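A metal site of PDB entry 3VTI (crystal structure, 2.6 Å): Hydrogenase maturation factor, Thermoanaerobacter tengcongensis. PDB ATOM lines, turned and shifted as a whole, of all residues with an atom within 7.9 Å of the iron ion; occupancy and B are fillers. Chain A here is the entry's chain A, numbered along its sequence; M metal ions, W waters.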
ATOM      1  N   TYR A 409     -29.539 -10.583 -18.572  1.00  0.00           N
ATOM      2  CA  TYR A 409     -30.541  -9.671 -19.093  1.00  0.00           C
ATOM      3  C   TYR A 409     -31.676 -10.442 -19.760  1.00  0.00           C
ATOM      4  O   TYR A 409     -31.450 -11.485 -20.380  1.00  0.00           O
ATOM      5  CB  TYR A 409     -29.928  -8.691 -20.097  1.00  0.00           C
ATOM      6  CG  TYR A 409     -28.758  -7.925 -19.542  1.00  0.00           C
ATOM      7  CD1 TYR A 409     -28.949  -6.799 -18.734  1.00  0.00           C
ATOM      8  CD2 TYR A 409     -27.433  -8.315 -19.832  1.00  0.00           C
ATOM      9  CE1 TYR A 409     -27.870  -6.107 -18.206  1.00  0.00           C
ATOM     10  CE2 TYR A 409     -26.354  -7.627 -19.328  1.00  0.00           C
ATOM     11  CZ  TYR A 409     -26.576  -6.528 -18.518  1.00  0.00           C
ATOM     12  OH  TYR A 409     -25.502  -5.834 -18.003  1.00  0.00           O
ATOM     13  N   ASP A 460     -24.345 -20.123 -18.766  1.00  0.00           N
ATOM     14  CA  ASP A 460     -23.371 -19.149 -19.250  1.00  0.00           C
ATOM     15  C   ASP A 460     -22.043 -19.273 -18.524  1.00  0.00           C
ATOM     16  O   ASP A 460     -21.978 -19.688 -17.360  1.00  0.00           O
ATOM     17  CB  ASP A 460     -23.912 -17.724 -19.103  1.00  0.00           C
ATOM     18  CG  ASP A 460     -23.223 -16.740 -20.030  1.00  0.00           C
ATOM     19  OD1 ASP A 460     -23.785 -16.464 -21.118  1.00  0.00           O
ATOM     20  OD2 ASP A 460     -22.114 -16.256 -19.687  1.00  0.00           O
ATOM     21  N   TYR A 465     -23.622 -14.604 -12.567  1.00  0.00           N
ATOM     22  CA  TYR A 465     -25.039 -14.643 -12.910  1.00  0.00           C
ATOM     23  C   TYR A 465     -25.801 -15.477 -11.891  1.00  0.00           C
ATOM     24  O   TYR A 465     -25.331 -16.545 -11.493  1.00  0.00           O
ATOM     25  CB  TYR A 465     -25.248 -15.311 -14.265  1.00  0.00           C
ATOM     26  CG  TYR A 465     -24.956 -14.474 -15.486  1.00  0.00           C
ATOM     27  CD1 TYR A 465     -24.291 -13.247 -15.406  1.00  0.00           C
ATOM     28  CD2 TYR A 465     -25.331 -14.937 -16.744  1.00  0.00           C
ATOM     29  CE1 TYR A 465     -24.021 -12.507 -16.555  1.00  0.00           C
ATOM     30  CE2 TYR A 465     -25.062 -14.209 -17.887  1.00  0.00           C
ATOM     31  CZ  TYR A 465     -24.424 -13.003 -17.790  1.00  0.00           C
ATOM     32  OH  TYR A 465     -24.175 -12.315 -18.955  1.00  0.00           O
ATOM     33  N   HIS A 483     -21.334 -17.117 -24.002  1.00  0.00           N
ATOM     34  CA  HIS A 483     -22.471 -16.240 -24.294  1.00  0.00           C
ATOM     35  C   HIS A 483     -22.761 -15.995 -25.772  1.00  0.00           C
ATOM     36  O   HIS A 483     -23.906 -16.114 -26.207  1.00  0.00           O
ATOM     37  CB  HIS A 483     -22.256 -14.899 -23.594  1.00  0.00           C
ATOM     38  CG  HIS A 483     -23.451 -13.999 -23.619  1.00  0.00           C
ATOM     39  ND1 HIS A 483     -24.490 -14.125 -22.734  1.00  0.00           N
ATOM     40  CD2 HIS A 483     -23.760 -12.959 -24.427  1.00  0.00           C
ATOM     41  CE1 HIS A 483     -25.406 -13.202 -22.993  1.00  0.00           C
ATOM     42  NE2 HIS A 483     -24.979 -12.475 -24.019  1.00  0.00           N
ATOM     43  N   HIS A 484     -21.734 -15.650 -26.542  1.00  0.00           N
ATOM     44  CA  HIS A 484     -21.936 -15.260 -27.948  1.00  0.00           C
ATOM     45  C   HIS A 484     -22.085 -16.456 -28.865  1.00  0.00           C
ATOM     46  O   HIS A 484     -22.807 -16.393 -29.863  1.00  0.00           O
ATOM     47  CB  HIS A 484     -20.843 -14.302 -28.403  1.00  0.00           C
ATOM     48  CG  HIS A 484     -20.801 -13.061 -27.578  1.00  0.00           C
ATOM     49  ND1 HIS A 484     -20.071 -12.964 -26.422  1.00  0.00           N
ATOM     50  CD2 HIS A 484     -21.480 -11.898 -27.698  1.00  0.00           C
ATOM     51  CE1 HIS A 484     -20.271 -11.782 -25.867  1.00  0.00           C
ATOM     52  NE2 HIS A 484     -21.127 -11.107 -26.616  1.00  0.00           N
ATOM     53  N   HIS A 487     -25.664 -17.150 -28.620  1.00  0.00           N
ATOM     54  CA  HIS A 487     -26.394 -16.291 -29.528  1.00  0.00           C
ATOM     55  C   HIS A 487     -26.445 -16.893 -30.935  1.00  0.00           C
ATOM     56  O   HIS A 487     -27.526 -17.077 -31.513  1.00  0.00           O
ATOM     57  CB  HIS A 487     -25.745 -14.901 -29.600  1.00  0.00           C
ATOM     58  CG  HIS A 487     -26.286 -13.928 -28.596  1.00  0.00           C
ATOM     59  ND1 HIS A 487     -27.630 -13.715 -28.408  1.00  0.00           N
ATOM     60  CD2 HIS A 487     -25.646 -13.082 -27.745  1.00  0.00           C
ATOM     61  CE1 HIS A 487     -27.802 -12.798 -27.473  1.00  0.00           C
ATOM     62  NE2 HIS A 487     -26.609 -12.391 -27.056  1.00  0.00           N
ATOM     63  N   ALA A 505     -21.730 -12.115 -33.830  1.00  0.00           N
ATOM     64  CA  ALA A 505     -22.343 -11.868 -32.529  1.00  0.00           C
ATOM     65  C   ALA A 505     -22.027 -10.470 -32.006  1.00  0.00           C
ATOM     66  O   ALA A 505     -20.962 -10.237 -31.428  1.00  0.00           O
ATOM     67  CB  ALA A 505     -21.909 -12.931 -31.546  1.00  0.00           C
ATOM     68  N   TYR A 506     -22.955  -9.547 -32.237  1.00  0.00           N
ATOM     69  CA  TYR A 506     -22.837  -8.152 -31.813  1.00  0.00           C
ATOM     70  C   TYR A 506     -23.868  -7.824 -30.724  1.00  0.00           C
ATOM     71  O   TYR A 506     -25.081  -7.930 -30.944  1.00  0.00           O
ATOM     72  CB  TYR A 506     -23.046  -7.185 -32.979  1.00  0.00           C
ATOM     73  CG  TYR A 506     -21.992  -7.184 -34.059  1.00  0.00           C
ATOM     74  CD1 TYR A 506     -20.793  -7.853 -33.907  1.00  0.00           C
ATOM     75  CD2 TYR A 506     -22.190  -6.445 -35.231  1.00  0.00           C
ATOM     76  CE1 TYR A 506     -19.815  -7.823 -34.916  1.00  0.00           C
ATOM     77  CE2 TYR A 506     -21.223  -6.406 -36.241  1.00  0.00           C
ATOM     78  CZ  TYR A 506     -20.051  -7.095 -36.073  1.00  0.00           C
ATOM     79  OH  TYR A 506     -19.123  -7.058 -37.065  1.00  0.00           O
ATOM     80  N   ASP A 507     -23.373  -7.417 -29.562  1.00  0.00           N
ATOM     81  CA  ASP A 507     -24.223  -6.928 -28.472  1.00  0.00           C
ATOM     82  C   ASP A 507     -23.418  -6.072 -27.498  1.00  0.00           C
ATOM     83  O   ASP A 507     -22.324  -5.600 -27.827  1.00  0.00           O
ATOM     84  CB  ASP A 507     -24.958  -8.083 -27.767  1.00  0.00           C
ATOM     85  CG  ASP A 507     -24.030  -9.006 -26.985  1.00  0.00           C
ATOM     86  OD1 ASP A 507     -22.805  -8.787 -26.947  1.00  0.00           O
ATOM     87  OD2 ASP A 507     -24.550  -9.973 -26.392  1.00  0.00           O
ATOM     88  N   GLY A 508     -23.969  -5.866 -26.311  1.00  0.00           N
ATOM     89  CA  GLY A 508     -23.325  -5.039 -25.308  1.00  0.00           C
ATOM     90  C   GLY A 508     -22.231  -5.781 -24.570  1.00  0.00           C
ATOM     91  O   GLY A 508     -21.081  -5.345 -24.530  1.00  0.00           O
ATOM     92  N   THR A 509     -22.564  -6.923 -23.976  1.00  0.00           N
ATOM     93  CA  THR A 509     -21.639  -7.581 -23.083  1.00  0.00           C
ATOM     94  C   THR A 509     -21.964  -9.032 -22.862  1.00  0.00           C
ATOM     95  O   THR A 509     -23.105  -9.441 -22.957  1.00  0.00           O
ATOM     96  CB  THR A 509     -21.565  -6.843 -21.732  1.00  0.00           C
ATOM     97  OG1 THR A 509     -20.720  -7.581 -20.840  1.00  0.00           O
ATOM     98  CG2 THR A 509     -22.932  -6.726 -21.126  1.00  0.00           C
ATOM     99  N   GLY A 510     -20.928  -9.795 -22.558  1.00  0.00           N
ATOM    100  CA  GLY A 510     -20.991 -11.217 -22.373  1.00  0.00           C
ATOM    101  C   GLY A 510     -19.583 -11.621 -21.994  1.00  0.00           C
ATOM    102  O   GLY A 510     -18.610 -11.098 -22.566  1.00  0.00           O
ATOM    103  N   TRP A 518     -16.909  -9.447 -24.215  1.00  0.00           N
ATOM    104  CA  TRP A 518     -17.101  -9.614 -25.662  1.00  0.00           C
ATOM    105  C   TRP A 518     -18.411  -8.954 -26.095  1.00  0.00           C
ATOM    106  O   TRP A 518     -19.176  -8.463 -25.264  1.00  0.00           O
ATOM    107  CB  TRP A 518     -17.023 -11.090 -26.071  1.00  0.00           C
ATOM    108  CG  TRP A 518     -15.693 -11.736 -25.952  1.00  0.00           C
ATOM    109  CD1 TRP A 518     -14.554 -11.225 -25.373  1.00  0.00           C
ATOM    110  CD2 TRP A 518     -15.359 -13.062 -26.380  1.00  0.00           C
ATOM    111  NE1 TRP A 518     -13.534 -12.144 -25.444  1.00  0.00           N
ATOM    112  CE2 TRP A 518     -14.001 -13.285 -26.049  1.00  0.00           C
ATOM    113  CE3 TRP A 518     -16.079 -14.092 -26.999  1.00  0.00           C
ATOM    114  CZ2 TRP A 518     -13.347 -14.482 -26.333  1.00  0.00           C
ATOM    115  CZ3 TRP A 518     -15.431 -15.282 -27.271  1.00  0.00           C
ATOM    116  CH2 TRP A 518     -14.086 -15.465 -26.942  1.00  0.00           C
ATOM    117  N   GLY A 519     -18.665  -8.960 -27.398  1.00  0.00           N
ATOM    118  CA  GLY A 519     -19.861  -8.331 -27.944  1.00  0.00           C
ATOM    119  C   GLY A 519     -19.690  -7.679 -29.308  1.00  0.00           C
ATOM    120  O   GLY A 519     -20.552  -6.909 -29.745  1.00  0.00           O
ATOM    121  N   SER A 700     -26.603 -12.598 -34.807  1.00  0.00           N
ATOM    122  CA  SER A 700     -27.313 -12.572 -33.540  1.00  0.00           C
ATOM    123  C   SER A 700     -26.631 -11.637 -32.519  1.00  0.00           C
ATOM    124  O   SER A 700     -25.620 -11.001 -32.813  1.00  0.00           O
ATOM    125  CB  SER A 700     -27.488 -13.989 -32.981  1.00  0.00           C
ATOM    126  OG  SER A 700     -28.563 -14.039 -32.049  1.00  0.00           O
ATOM    127  N   GLY A 701     -27.199 -11.565 -31.318  1.00  0.00           N
ATOM    128  CA  GLY A 701     -26.817 -10.570 -30.346  1.00  0.00           C
ATOM    129  C   GLY A 701     -27.744  -9.371 -30.425  1.00  0.00           C
ATOM    130  O   GLY A 701     -28.197  -9.002 -31.507  1.00  0.00           O
ATOM    131  N   GLY A 702     -27.982  -8.748 -29.268  1.00  0.00           N
ATOM    132  CA  GLY A 702     -28.861  -7.604 -29.110  1.00  0.00           C
ATOM    133  C   GLY A 702     -28.712  -6.465 -30.102  1.00  0.00           C
ATOM    134  O   GLY A 702     -29.709  -5.801 -30.402  1.00  0.00           O
ATOM    135  N   SER A 703     -27.503  -6.240 -30.607  1.00  0.00           N
ATOM    136  CA  SER A 703     -27.252  -5.138 -31.549  1.00  0.00           C
ATOM    137  C   SER A 703     -28.130  -5.229 -32.794  1.00  0.00           C
ATOM    138  O   SER A 703     -28.433  -4.212 -33.428  1.00  0.00           O
ATOM    139  CB  SER A 703     -25.777  -5.081 -31.977  1.00  0.00           C
ATOM    140  OG  SER A 703     -24.939  -4.765 -30.894  1.00  0.00           O
ATOM    141  N   CYS A 732     -32.950 -12.008 -30.886  1.00  0.00           N
ATOM    142  CA  CYS A 732     -31.502 -11.946 -31.041  1.00  0.00           C
ATOM    143  C   CYS A 732     -30.849 -11.390 -29.767  1.00  0.00           C
ATOM    144  O   CYS A 732     -29.652 -11.484 -29.599  1.00  0.00           O
ATOM    145  CB  CYS A 732     -31.102 -11.133 -32.284  1.00  0.00           C
ATOM    146  SG  CYS A 732     -31.496  -9.363 -32.221  1.00  0.00           S
ATOM    147  N   ASN A 733     -31.657 -10.825 -28.848  1.00  0.00           N
ATOM    148  CA  ASN A 733     -31.115 -10.406 -27.540  1.00  0.00           C
ATOM    149  C   ASN A 733     -31.008 -11.587 -26.555  1.00  0.00           C
ATOM    150  O   ASN A 733     -31.268 -12.730 -26.924  1.00  0.00           O
ATOM    151  CB  ASN A 733     -31.916  -9.248 -26.944  1.00  0.00           C
ATOM    152  CG  ASN A 733     -33.381  -9.623 -26.656  1.00  0.00           C
ATOM    153  OD1 ASN A 733     -33.673 -10.688 -26.121  1.00  0.00           O
ATOM    154  ND2 ASN A 733     -34.289  -8.712 -26.984  1.00  0.00           N
ATOM    155  N   ASP A 734     -30.662 -11.297 -25.299  1.00  0.00           N
ATOM    156  CA  ASP A 734     -30.408 -12.351 -24.327  1.00  0.00           C
ATOM    157  C   ASP A 734     -31.630 -13.189 -23.981  1.00  0.00           C
ATOM    158  O   ASP A 734     -31.531 -14.161 -23.231  1.00  0.00           O
ATOM    159  CB  ASP A 734     -29.772 -11.784 -23.067  1.00  0.00           C
ATOM    160  CG  ASP A 734     -28.379 -11.254 -23.318  1.00  0.00           C
ATOM    161  OD1 ASP A 734     -27.941 -11.245 -24.486  1.00  0.00           O
ATOM    162  OD2 ASP A 734     -27.735 -10.843 -22.334  1.00  0.00           O
ATOM    163  N   GLY A 735     -32.784 -12.818 -24.521  1.00  0.00           N
ATOM    164  CA  GLY A 735     -33.991 -13.635 -24.399  1.00  0.00           C
ATOM    165  C   GLY A 735     -33.911 -14.942 -25.165  1.00  0.00           C
ATOM    166  O   GLY A 735     -34.669 -15.865 -24.873  1.00  0.00           O
ATOM    167  N   ILE A 737     -30.904 -16.671 -25.595  1.00  0.00           N
ATOM    168  CA  ILE A 737     -29.652 -17.330 -25.207  1.00  0.00           C
ATOM    169  C   ILE A 737     -29.882 -18.778 -24.769  1.00  0.00           C
ATOM    170  O   ILE A 737     -29.137 -19.678 -25.152  1.00  0.00           O
ATOM    171  CB  ILE A 737     -28.925 -16.496 -24.090  1.00  0.00           C
ATOM    172  CG1 ILE A 737     -28.211 -15.285 -24.705  1.00  0.00           C
ATOM    173  CG2 ILE A 737     -27.970 -17.351 -23.230  1.00  0.00           C
ATOM    174  CD1 ILE A 737     -27.100 -15.631 -25.669  1.00  0.00           C
HETATM  175 FE    FE M   1     -26.059 -10.905 -25.357  1.00  0.00          FE
HETATM  176  O   HOH W   1     -27.522  -9.217 -26.317  1.00  0.00           O
HETATM  177  O   HOH W   2     -26.023  -9.421 -23.675  1.00  0.00           O
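Four residues have an atom within 4 Å of the iron ion: His 483, His 487, Asp 507 and Asp 734.
The nearest printed residue that does not touch the iron ion is Thr 509 (4.1 Å).
Water W2 lies within hydrogen-bond range of the side-chain carboxylate of Asp 734 (2.6 Å) and the backbone carbonyl oxygen of Thr 509 (3.0 Å).
OD2 of Asp 507 is bound to the iron ion (2.1 Å).
OD1 of Asp 734 binds the iron ion (2.1 Å).
The iron ion is bound by water W2, at 2.2 Å.
A ring nitrogen (NE2) of His 487 binds the iron ion, 2.3 Å away.
NE2 of His 483 is bound to the iron ion, 2.3 Å away.
Water W1 binds the iron ion, 2.4 Å away.
The iron ion has six donor atoms within binding distance.
The side-chain carboxylate (OD1) of Asp 507 lies within hydrogen-bond range of a ring nitrogen (NE2) of His 484 (2.9 Å).
N of Asp 507 lies close to OG of Ser 703 (3.4 Å).
The backbone NH (N) of Asp 507 lies within hydrogen-bond range of the backbone carbonyl oxygen (O) of Gly 519.
ND1 of His 487 sits close to O of Cys 732 (3.2 Å).
OG of Ser 700 is in hydrogen-bond range of O of His 487 (3.3 Å).
A ring nitrogen (ND1) of His 483 is in hydrogen-bond range of the side-chain carboxylate (OD1) of Asp 460, at 2.9 Å.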
